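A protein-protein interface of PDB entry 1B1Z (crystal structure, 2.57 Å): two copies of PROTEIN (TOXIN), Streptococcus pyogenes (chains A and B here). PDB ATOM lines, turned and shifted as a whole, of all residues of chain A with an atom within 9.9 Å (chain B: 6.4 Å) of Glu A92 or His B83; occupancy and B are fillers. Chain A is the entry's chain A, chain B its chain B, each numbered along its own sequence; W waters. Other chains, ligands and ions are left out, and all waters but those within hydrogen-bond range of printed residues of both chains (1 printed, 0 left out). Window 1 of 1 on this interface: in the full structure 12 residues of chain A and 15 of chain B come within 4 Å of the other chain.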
ATOM      1  N   ASN A  47      15.521  33.191  32.995  1.00  0.00           N
ATOM      2  CA  ASN A  47      14.859  32.031  33.593  1.00  0.00           C
ATOM      3  C   ASN A  47      13.381  32.264  33.368  1.00  0.00           C
ATOM      4  O   ASN A  47      12.654  32.660  34.277  1.00  0.00           O
ATOM      5  CB  ASN A  47      15.118  31.952  35.100  1.00  0.00           C
ATOM      6  CG  ASN A  47      16.538  31.532  35.433  1.00  0.00           C
ATOM      7  OD1 ASN A  47      17.118  32.003  36.415  1.00  0.00           O
ATOM      8  ND2 ASN A  47      17.108  30.642  34.618  1.00  0.00           N
ATOM      9  N   VAL A  48      12.938  32.032  32.147  1.00  0.00           N
ATOM     10  CA  VAL A  48      11.548  32.254  31.819  1.00  0.00           C
ATOM     11  C   VAL A  48      11.014  30.974  31.210  1.00  0.00           C
ATOM     12  O   VAL A  48      11.761  30.231  30.586  1.00  0.00           O
ATOM     13  CB  VAL A  48      11.425  33.435  30.823  1.00  0.00           C
ATOM     14  CG1 VAL A  48      11.770  34.745  31.534  1.00  0.00           C
ATOM     15  CG2 VAL A  48      12.372  33.228  29.635  1.00  0.00           C
ATOM     16  N   SER A  49       9.729  30.708  31.382  1.00  0.00           N
ATOM     17  CA  SER A  49       9.174  29.484  30.847  1.00  0.00           C
ATOM     18  C   SER A  49       8.128  29.647  29.768  1.00  0.00           C
ATOM     19  O   SER A  49       7.596  30.725  29.541  1.00  0.00           O
ATOM     20  CB  SER A  49       8.589  28.654  31.978  1.00  0.00           C
ATOM     21  OG  SER A  49       9.607  28.285  32.884  1.00  0.00           O
ATOM     22  N   GLY A  50       7.842  28.536  29.109  1.00  0.00           N
ATOM     23  CA  GLY A  50       6.847  28.500  28.060  1.00  0.00           C
ATOM     24  C   GLY A  50       6.747  27.041  27.682  1.00  0.00           C
ATOM     25  O   GLY A  50       7.529  26.234  28.189  1.00  0.00           O
ATOM     26  N   ASN A  52       7.823  23.925  26.180  1.00  0.00           N
ATOM     27  CA  ASN A  52       9.076  23.545  25.533  1.00  0.00           C
ATOM     28  C   ASN A  52      10.334  24.183  26.096  1.00  0.00           C
ATOM     29  O   ASN A  52      11.427  23.844  25.650  1.00  0.00           O
ATOM     30  CB  ASN A  52       9.036  23.817  24.028  1.00  0.00           C
ATOM     31  CG  ASN A  52       7.915  23.077  23.331  1.00  0.00           C
ATOM     32  OD1 ASN A  52       7.399  22.076  23.843  1.00  0.00           O
ATOM     33  ND2 ASN A  52       7.527  23.564  22.150  1.00  0.00           N
ATOM     34  N   TYR A  53      10.210  25.098  27.056  1.00  0.00           N
ATOM     35  CA  TYR A  53      11.412  25.712  27.627  1.00  0.00           C
ATOM     36  C   TYR A  53      11.272  26.344  29.007  1.00  0.00           C
ATOM     37  O   TYR A  53      10.242  26.931  29.349  1.00  0.00           O
ATOM     38  CB  TYR A  53      11.997  26.745  26.656  1.00  0.00           C
ATOM     39  CG  TYR A  53      11.203  28.023  26.544  1.00  0.00           C
ATOM     40  CD1 TYR A  53      11.451  29.098  27.395  1.00  0.00           C
ATOM     41  CD2 TYR A  53      10.222  28.170  25.563  1.00  0.00           C
ATOM     42  CE1 TYR A  53      10.748  30.279  27.273  1.00  0.00           C
ATOM     43  CE2 TYR A  53       9.514  29.349  25.433  1.00  0.00           C
ATOM     44  CZ  TYR A  53       9.781  30.399  26.289  1.00  0.00           C
ATOM     45  OH  TYR A  53       9.073  31.573  26.157  1.00  0.00           O
ATOM     46  N   ASP A  54      12.334  26.219  29.795  1.00  0.00           N
ATOM     47  CA  ASP A  54      12.373  26.762  31.143  1.00  0.00           C
ATOM     48  C   ASP A  54      13.547  27.733  31.253  1.00  0.00           C
ATOM     49  O   ASP A  54      13.835  28.261  32.322  1.00  0.00           O
ATOM     50  CB  ASP A  54      12.536  25.625  32.163  1.00  0.00           C
ATOM     51  CG  ASP A  54      11.378  24.622  32.128  1.00  0.00           C
ATOM     52  OD1 ASP A  54      10.228  25.018  32.429  1.00  0.00           O
ATOM     53  OD2 ASP A  54      11.618  23.435  31.803  1.00  0.00           O
ATOM     54  N   LYS A  55      14.222  27.954  30.132  1.00  0.00           N
ATOM     55  CA  LYS A  55      15.362  28.859  30.065  1.00  0.00           C
ATOM     56  C   LYS A  55      15.351  29.485  28.679  1.00  0.00           C
ATOM     57  O   LYS A  55      14.984  28.830  27.707  1.00  0.00           O
ATOM     58  CB  LYS A  55      16.673  28.094  30.253  1.00  0.00           C
ATOM     59  CG  LYS A  55      17.155  28.023  31.688  1.00  0.00           C
ATOM     60  CD  LYS A  55      18.673  27.916  31.748  1.00  0.00           C
ATOM     61  CE  LYS A  55      19.209  28.338  33.119  1.00  0.00           C
ATOM     62  NZ  LYS A  55      18.164  28.265  34.189  1.00  0.00           N
ATOM     63  N   LEU A  56      15.747  30.751  28.586  1.00  0.00           N
ATOM     64  CA  LEU A  56      15.775  31.426  27.302  1.00  0.00           C
ATOM     65  C   LEU A  56      17.056  32.220  27.102  1.00  0.00           C
ATOM     66  O   LEU A  56      17.454  33.014  27.958  1.00  0.00           O
ATOM     67  CB  LEU A  56      14.567  32.357  27.167  1.00  0.00           C
ATOM     68  CG  LEU A  56      14.634  33.362  26.012  1.00  0.00           C
ATOM     69  CD1 LEU A  56      14.382  32.663  24.685  1.00  0.00           C
ATOM     70  CD2 LEU A  56      13.619  34.447  26.249  1.00  0.00           C
ATOM     71  N   TYR A  82      15.245  25.608  18.539  1.00  0.00           N
ATOM     72  CA  TYR A  82      15.788  24.687  19.520  1.00  0.00           C
ATOM     73  C   TYR A  82      17.007  23.930  19.025  1.00  0.00           C
ATOM     74  O   TYR A  82      17.996  23.826  19.741  1.00  0.00           O
ATOM     75  CB  TYR A  82      14.689  23.724  19.960  1.00  0.00           C
ATOM     76  CG  TYR A  82      13.477  24.436  20.525  1.00  0.00           C
ATOM     77  CD1 TYR A  82      12.384  24.745  19.717  1.00  0.00           C
ATOM     78  CD2 TYR A  82      13.440  24.832  21.860  1.00  0.00           C
ATOM     79  CE1 TYR A  82      11.280  25.435  20.222  1.00  0.00           C
ATOM     80  CE2 TYR A  82      12.343  25.523  22.376  1.00  0.00           C
ATOM     81  CZ  TYR A  82      11.268  25.821  21.552  1.00  0.00           C
ATOM     82  OH  TYR A  82      10.184  26.502  22.067  1.00  0.00           O
ATOM     83  N   HIS A  83      16.949  23.407  17.805  1.00  0.00           N
ATOM     84  CA  HIS A  83      18.090  22.678  17.248  1.00  0.00           C
ATOM     85  C   HIS A  83      19.291  23.619  17.080  1.00  0.00           C
ATOM     86  O   HIS A  83      19.188  24.666  16.432  1.00  0.00           O
ATOM     87  CB  HIS A  83      17.721  22.052  15.897  1.00  0.00           C
ATOM     88  CG  HIS A  83      18.899  21.533  15.128  1.00  0.00           C
ATOM     89  ND1 HIS A  83      19.270  22.042  13.901  1.00  0.00           N
ATOM     90  CD2 HIS A  83      19.794  20.559  15.418  1.00  0.00           C
ATOM     91  CE1 HIS A  83      20.343  21.404  13.468  1.00  0.00           C
ATOM     92  NE2 HIS A  83      20.681  20.500  14.370  1.00  0.00           N
ATOM     93  N   LEU A  84      20.422  23.225  17.662  1.00  0.00           N
ATOM     94  CA  LEU A  84      21.657  24.004  17.622  1.00  0.00           C
ATOM     95  C   LEU A  84      21.598  25.117  18.670  1.00  0.00           C
ATOM     96  O   LEU A  84      22.215  26.177  18.518  1.00  0.00           O
ATOM     97  CB  LEU A  84      21.886  24.601  16.229  1.00  0.00           C
ATOM     98  CG  LEU A  84      22.009  23.617  15.059  1.00  0.00           C
ATOM     99  CD1 LEU A  84      22.557  24.343  13.844  1.00  0.00           C
ATOM    100  CD2 LEU A  84      22.913  22.453  15.443  1.00  0.00           C
ATOM    101  N   CYS A  85      20.833  24.862  19.727  1.00  0.00           N
ATOM    102  CA  CYS A  85      20.683  25.791  20.840  1.00  0.00           C
ATOM    103  C   CYS A  85      21.155  25.015  22.074  1.00  0.00           C
ATOM    104  O   CYS A  85      20.340  24.493  22.841  1.00  0.00           O
ATOM    105  CB  CYS A  85      19.211  26.201  20.990  1.00  0.00           C
ATOM    106  SG  CYS A  85      18.820  27.257  22.430  1.00  0.00           S
ATOM    107  N   TYR A  86      22.473  24.919  22.245  1.00  0.00           N
ATOM    108  CA  TYR A  86      23.047  24.190  23.376  1.00  0.00           C
ATOM    109  C   TYR A  86      23.487  25.156  24.474  1.00  0.00           C
ATOM    110  O   TYR A  86      24.126  26.170  24.191  1.00  0.00           O
ATOM    111  CB  TYR A  86      24.240  23.335  22.910  1.00  0.00           C
ATOM    112  N   LEU A  87      23.141  24.838  25.721  1.00  0.00           N
ATOM    113  CA  LEU A  87      23.509  25.675  26.862  1.00  0.00           C
ATOM    114  C   LEU A  87      24.655  25.052  27.680  1.00  0.00           C
ATOM    115  O   LEU A  87      25.599  25.747  28.066  1.00  0.00           O
ATOM    116  CB  LEU A  87      22.286  25.915  27.759  1.00  0.00           C
ATOM    117  CG  LEU A  87      21.855  27.366  28.009  1.00  0.00           C
ATOM    118  CD1 LEU A  87      21.626  28.082  26.690  1.00  0.00           C
ATOM    119  CD2 LEU A  87      20.586  27.376  28.847  1.00  0.00           C
ATOM    120  N   CYS A  88      24.570  23.749  27.947  1.00  0.00           N
ATOM    121  CA  CYS A  88      25.619  23.056  28.697  1.00  0.00           C
ATOM    122  C   CYS A  88      25.450  21.536  28.766  1.00  0.00           C
ATOM    123  O   CYS A  88      25.863  20.914  29.742  1.00  0.00           O
ATOM    124  CB  CYS A  88      25.746  23.630  30.122  1.00  0.00           C
ATOM    125  SG  CYS A  88      24.199  24.046  30.984  1.00  0.00           S
ATOM    126  N   GLU A  89      24.854  20.953  27.725  1.00  0.00           N
ATOM    127  CA  GLU A  89      24.622  19.501  27.623  1.00  0.00           C
ATOM    128  C   GLU A  89      23.504  18.932  28.511  1.00  0.00           C
ATOM    129  O   GLU A  89      22.893  17.920  28.165  1.00  0.00           O
ATOM    130  CB  GLU A  89      25.919  18.723  27.892  1.00  0.00           C
ATOM    131  CG  GLU A  89      25.964  17.329  27.249  1.00  0.00           C
ATOM    132  CD  GLU A  89      25.757  16.182  28.249  1.00  0.00           C
ATOM    133  OE1 GLU A  89      26.717  15.418  28.501  1.00  0.00           O
ATOM    134  OE2 GLU A  89      24.632  16.039  28.779  1.00  0.00           O
ATOM    135  N   ASN A  90      23.247  19.565  29.655  1.00  0.00           N
ATOM    136  CA  ASN A  90      22.191  19.106  30.561  1.00  0.00           C
ATOM    137  C   ASN A  90      21.121  20.186  30.751  1.00  0.00           C
ATOM    138  O   ASN A  90      20.389  20.194  31.747  1.00  0.00           O
ATOM    139  CB  ASN A  90      22.781  18.710  31.919  1.00  0.00           C
ATOM    140  CG  ASN A  90      23.061  19.909  32.815  1.00  0.00           C
ATOM    141  OD1 ASN A  90      23.251  21.034  32.340  1.00  0.00           O
ATOM    142  ND2 ASN A  90      23.093  19.670  34.125  1.00  0.00           N
ATOM    143  N   ALA A  91      21.049  21.104  29.791  1.00  0.00           N
ATOM    144  CA  ALA A  91      20.070  22.180  29.827  1.00  0.00           C
ATOM    145  C   ALA A  91      19.010  21.857  28.791  1.00  0.00           C
ATOM    146  O   ALA A  91      18.986  22.432  27.702  1.00  0.00           O
ATOM    147  CB  ALA A  91      20.729  23.521  29.513  1.00  0.00           C
ATOM    148  N   GLU A  92      18.162  20.891  29.126  1.00  0.00           N
ATOM    149  CA  GLU A  92      17.071  20.496  28.254  1.00  0.00           C
ATOM    150  C   GLU A  92      16.040  21.562  28.527  1.00  0.00           C
ATOM    151  O   GLU A  92      16.165  22.309  29.507  1.00  0.00           O
ATOM    152  CB  GLU A  92      16.531  19.131  28.655  1.00  0.00           C
ATOM    153  CG  GLU A  92      17.496  17.998  28.385  1.00  0.00           C
ATOM    154  CD  GLU A  92      17.391  16.885  29.397  1.00  0.00           C
ATOM    155  OE1 GLU A  92      16.755  17.086  30.449  1.00  0.00           O
ATOM    156  OE2 GLU A  92      17.950  15.805  29.140  1.00  0.00           O
ATOM    157  N   ARG A  93      15.026  21.650  27.680  1.00  0.00           N
ATOM    158  CA  ARG A  93      14.000  22.672  27.865  1.00  0.00           C
ATOM    159  C   ARG A  93      14.632  24.071  27.807  1.00  0.00           C
ATOM    160  O   ARG A  93      14.398  24.913  28.670  1.00  0.00           O
ATOM    161  CB  ARG A  93      13.280  22.457  29.201  1.00  0.00           C
ATOM    162  CG  ARG A  93      12.803  21.031  29.411  1.00  0.00           C
ATOM    163  CD  ARG A  93      11.338  20.862  29.067  1.00  0.00           C
ATOM    164  NE  ARG A  93      10.501  21.721  29.893  1.00  0.00           N
ATOM    165  CZ  ARG A  93       9.344  22.235  29.492  1.00  0.00           C
ATOM    166  NH1 ARG A  93       8.898  21.965  28.276  1.00  0.00           N
ATOM    167  NH2 ARG A  93       8.649  23.034  30.295  1.00  0.00           N
ATOM    168  N   SER A  94      15.441  24.291  26.773  1.00  0.00           N
ATOM    169  CA  SER A  94      16.125  25.561  26.529  1.00  0.00           C
ATOM    170  C   SER A  94      15.737  26.085  25.143  1.00  0.00           C
ATOM    171  O   SER A  94      15.635  25.310  24.188  1.00  0.00           O
ATOM    172  CB  SER A  94      17.644  25.366  26.574  1.00  0.00           C
ATOM    173  OG  SER A  94      18.121  25.386  27.906  1.00  0.00           O
ATOM    174  N   ALA A  95      15.528  27.396  25.038  1.00  0.00           N
ATOM    175  CA  ALA A  95      15.158  28.018  23.767  1.00  0.00           C
ATOM    176  C   ALA A  95      16.156  29.117  23.419  1.00  0.00           C
ATOM    177  O   ALA A  95      16.836  29.648  24.291  1.00  0.00           O
ATOM    178  CB  ALA A  95      13.743  28.597  23.846  1.00  0.00           C
ATOM    179  N   ASN B  18      11.508  17.793  34.327  1.00  0.00           N
ATOM    180  CA  ASN B  18      11.893  17.289  33.015  1.00  0.00           C
ATOM    181  C   ASN B  18      11.373  15.856  32.839  1.00  0.00           C
ATOM    182  O   ASN B  18      11.293  15.349  31.726  1.00  0.00           O
ATOM    183  CB  ASN B  18      13.418  17.360  32.846  1.00  0.00           C
ATOM    184  CG  ASN B  18      13.923  18.798  32.678  1.00  0.00           C
ATOM    185  OD1 ASN B  18      13.145  19.710  32.415  1.00  0.00           O
ATOM    186  ND2 ASN B  18      15.229  18.996  32.827  1.00  0.00           N
ATOM    187  N   TYR B  81      12.111  12.504  23.404  1.00  0.00           N
ATOM    188  CA  TYR B  81      12.903  13.592  23.924  1.00  0.00           C
ATOM    189  C   TYR B  81      13.489  14.228  22.675  1.00  0.00           C
ATOM    190  O   TYR B  81      13.512  13.604  21.612  1.00  0.00           O
ATOM    191  CB  TYR B  81      13.998  13.079  24.861  1.00  0.00           C
ATOM    192  CG  TYR B  81      15.077  12.247  24.211  1.00  0.00           C
ATOM    193  CD1 TYR B  81      16.229  12.843  23.700  1.00  0.00           C
ATOM    194  CD2 TYR B  81      14.970  10.855  24.146  1.00  0.00           C
ATOM    195  CE1 TYR B  81      17.250  12.075  23.139  1.00  0.00           C
ATOM    196  CE2 TYR B  81      15.988  10.076  23.588  1.00  0.00           C
ATOM    197  CZ  TYR B  81      17.123  10.696  23.088  1.00  0.00           C
ATOM    198  OH  TYR B  81      18.138   9.941  22.541  1.00  0.00           O
ATOM    199  N   TYR B  82      13.941  15.470  22.803  1.00  0.00           N
ATOM    200  CA  TYR B  82      14.502  16.212  21.684  1.00  0.00           C
ATOM    201  C   TYR B  82      15.923  16.671  21.951  1.00  0.00           C
ATOM    202  O   TYR B  82      16.758  16.677  21.054  1.00  0.00           O
ATOM    203  CB  TYR B  82      13.614  17.417  21.389  1.00  0.00           C
ATOM    204  CG  TYR B  82      12.170  17.040  21.129  1.00  0.00           C
ATOM    205  CD1 TYR B  82      11.258  16.929  22.182  1.00  0.00           C
ATOM    206  CD2 TYR B  82      11.728  16.741  19.839  1.00  0.00           C
ATOM    207  CE1 TYR B  82       9.951  16.524  21.955  1.00  0.00           C
ATOM    208  CE2 TYR B  82      10.429  16.336  19.606  1.00  0.00           C
ATOM    209  CZ  TYR B  82       9.547  16.228  20.666  1.00  0.00           C
ATOM    210  OH  TYR B  82       8.258  15.800  20.439  1.00  0.00           O
ATOM    211  N   HIS B  83      16.202  17.062  23.187  1.00  0.00           N
ATOM    212  CA  HIS B  83      17.544  17.507  23.533  1.00  0.00           C
ATOM    213  C   HIS B  83      18.538  16.351  23.433  1.00  0.00           C
ATOM    214  O   HIS B  83      18.341  15.303  24.049  1.00  0.00           O
ATOM    215  CB  HIS B  83      17.568  18.079  24.948  1.00  0.00           C
ATOM    216  CG  HIS B  83      18.918  18.565  25.366  1.00  0.00           C
ATOM    217  ND1 HIS B  83      19.631  17.991  26.398  1.00  0.00           N
ATOM    218  CD2 HIS B  83      19.697  19.562  24.879  1.00  0.00           C
ATOM    219  CE1 HIS B  83      20.789  18.614  26.529  1.00  0.00           C
ATOM    220  NE2 HIS B  83      20.855  19.571  25.620  1.00  0.00           N
ATOM    221  N   LEU B  84      19.602  16.555  22.663  1.00  0.00           N
ATOM    222  CA  LEU B  84      20.651  15.550  22.455  1.00  0.00           C
ATOM    223  C   LEU B  84      20.212  14.511  21.417  1.00  0.00           C
ATOM    224  O   LEU B  84      20.840  13.455  21.267  1.00  0.00           O
ATOM    225  CB  LEU B  84      21.016  14.843  23.776  1.00  0.00           C
ATOM    226  CG  LEU B  84      21.637  15.671  24.913  1.00  0.00           C
ATOM    227  CD1 LEU B  84      22.194  14.754  26.004  1.00  0.00           C
ATOM    228  CD2 LEU B  84      22.736  16.558  24.351  1.00  0.00           C
ATOM    229  N   CYS B  85      19.133  14.813  20.702  1.00  0.00           N
ATOM    230  CA  CYS B  85      18.632  13.904  19.688  1.00  0.00           C
ATOM    231  C   CYS B  85      19.299  14.236  18.360  1.00  0.00           C
ATOM    232  O   CYS B  85      18.645  14.318  17.318  1.00  0.00           O
ATOM    233  CB  CYS B  85      17.112  14.036  19.582  1.00  0.00           C
ATOM    234  SG  CYS B  85      16.339  13.044  18.267  1.00  0.00           S
ATOM    235  N   TYR B  86      20.618  14.418  18.409  1.00  0.00           N
ATOM    236  CA  TYR B  86      21.413  14.767  17.227  1.00  0.00           C
ATOM    237  C   TYR B  86      21.239  13.801  16.065  1.00  0.00           C
ATOM    238  O   TYR B  86      21.477  12.596  16.196  1.00  0.00           O
ATOM    239  CB  TYR B  86      22.902  14.866  17.596  1.00  0.00           C
ATOM    240  N   PHE B 190      20.324  14.306  35.913  1.00  0.00           N
ATOM    241  CA  PHE B 190      20.066  13.341  34.857  1.00  0.00           C
ATOM    242  C   PHE B 190      19.793  14.048  33.545  1.00  0.00           C
ATOM    243  O   PHE B 190      19.761  15.274  33.466  1.00  0.00           O
ATOM    244  CB  PHE B 190      18.839  12.501  35.224  1.00  0.00           C
ATOM    245  CG  PHE B 190      17.548  13.293  35.239  1.00  0.00           C
ATOM    246  CD1 PHE B 190      16.682  13.265  34.141  1.00  0.00           C
ATOM    247  CD2 PHE B 190      17.226  14.105  36.326  1.00  0.00           C
ATOM    248  CE1 PHE B 190      15.527  14.034  34.123  1.00  0.00           C
ATOM    249  CE2 PHE B 190      16.069  14.879  36.316  1.00  0.00           C
ATOM    250  CZ  PHE B 190      15.219  14.844  35.211  1.00  0.00           C
ATOM    251  N   THR B 191      19.562  13.247  32.519  1.00  0.00           N
ATOM    252  CA  THR B 191      19.276  13.744  31.192  1.00  0.00           C
ATOM    253  C   THR B 191      18.089  12.905  30.718  1.00  0.00           C
ATOM    254  O   THR B 191      17.998  11.719  31.034  1.00  0.00           O
ATOM    255  CB  THR B 191      20.529  13.544  30.299  1.00  0.00           C
ATOM    256  OG1 THR B 191      21.031  14.822  29.892  1.00  0.00           O
ATOM    257  CG2 THR B 191      20.224  12.701  29.083  1.00  0.00           C
ATOM    258  N   GLN B 192      17.158  13.512  29.999  1.00  0.00           N
ATOM    259  CA  GLN B 192      16.015  12.765  29.504  1.00  0.00           C
ATOM    260  C   GLN B 192      16.538  11.617  28.653  1.00  0.00           C
ATOM    261  O   GLN B 192      16.066  10.487  28.749  1.00  0.00           O
ATOM    262  CB  GLN B 192      15.112  13.663  28.648  1.00  0.00           C
ATOM    263  CG  GLN B 192      13.940  14.258  29.405  1.00  0.00           C
ATOM    264  CD  GLN B 192      13.494  15.596  28.852  1.00  0.00           C
ATOM    265  OE1 GLN B 192      13.854  15.968  27.741  1.00  0.00           O
ATOM    266  NE2 GLN B 192      12.704  16.326  29.631  1.00  0.00           N
ATOM    267  N   SER B 193      17.537  11.916  27.833  1.00  0.00           N
ATOM    268  CA  SER B 193      18.117  10.929  26.927  1.00  0.00           C
ATOM    269  C   SER B 193      18.860   9.754  27.564  1.00  0.00           C
ATOM    270  O   SER B 193      19.055   8.727  26.917  1.00  0.00           O
ATOM    271  CB  SER B 193      19.034  11.631  25.931  1.00  0.00           C
ATOM    272  OG  SER B 193      20.376  11.303  26.180  1.00  0.00           O
ATOM    273  N   LYS B 194      19.283   9.900  28.817  1.00  0.00           N
ATOM    274  CA  LYS B 194      19.988   8.830  29.508  1.00  0.00           C
ATOM    275  C   LYS B 194      18.991   8.073  30.348  1.00  0.00           C
ATOM    276  O   LYS B 194      19.074   6.853  30.476  1.00  0.00           O
ATOM    277  CB  LYS B 194      21.088   9.392  30.410  1.00  0.00           C
ATOM    278  CG  LYS B 194      22.268   9.954  29.636  1.00  0.00           C
ATOM    279  CD  LYS B 194      23.539   9.161  29.849  1.00  0.00           C
ATOM    280  CE  LYS B 194      24.768  10.069  29.766  1.00  0.00           C
ATOM    281  NZ  LYS B 194      24.525  11.287  28.918  1.00  0.00           N
HETATM  282  O   HOH W   1      18.578  14.357  27.028  1.00  0.00           O
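The side-chain carboxylate (OE1) of Glu A92 lies within hydrogen-bond range of the side-chain amide nitrogen (ND2) of Asn B18 (3.4 Å).
The side-chain carboxylate (OE2) of Glu A92 lies close to the side-chain hydroxyl (OG1) of Thr B191, at 3.3 Å.
N of Gln B192 lies within hydrogen-bond range of OE2 of Glu A92, at 2.6 Å.
The side-chain carboxylate (OD2) of Asp A54 is in salt-bridge range of the guanidinium group (NE) of Arg A93, at 2.8 Å.
O of Arg A93 lies within hydrogen-bond range of N of Lys A55 (3.4 Å).
The backbone carbonyl oxygen (O) of Asn B18 is in hydrogen-bond range of the side-chain amide nitrogen (NE2) of Gln B192 (2.7 Å).
His B83 touches Glu A89 (CE1 to O, 2.8 Å).
CD1 of Leu B84 touches O of Glu A89, at 3.9 Å.
Glu A89 touches Thr B191.
CG of Glu A92 touches ND1 of His B83, 2.9 Å away.
Asn B18 touches Arg A93.
Of the printed residues of chain B, Glu A89 touches His B83, Leu B84 and Thr B191.
Of the printed residues of chain B, Glu A92 touches Asn B18 (3.4 Å), His B83 (2.9 Å), Thr B191 (3.2 Å) and Gln B192 (2.6 Å).
Of the printed residues of chain B, Arg A93 touches Asn B18 (3.3 Å).
Printed residues of chain A within 4 Å of Asn B18: Glu A92 (3.4 Å) and Arg A93 (3.3 Å).
Tyr B82 touches none of the printed residues of chain A.
Of the printed residues of chain A, His B83 touches Glu A89 and Glu A92.
Thr B191 touches two residues of chain A.
Gln B192 touches one residue of chain A.
The nearest residue of chain B that does not touch Glu A92 is Ser B193 (4.1 Å).
The nearest printed residue of chain A that does not touch His B83 is Ala A91 (4.002 Å).
The nearest printed residue of chain A that does not touch Asn B18 is Asp A54 (4.1 Å).
Of the 23 printed residues of chain A, 3 touch a printed residue of chain B.
Among the printed residues, no Asp or Glu carboxylate lies within 4 Å of a Lys or Arg side-chain nitrogen of the other chain.
Positions printed for both chains: 82, 83, 84, 85 and 86.
Of the 8 pairs that touch across the chains among the printed residues, none has its exchanged pair printed and touching as well.
Water W1 lies within hydrogen-bond range of OE2 of Glu A92, N of Ser B193, O of His B83 and N of Gln B192.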
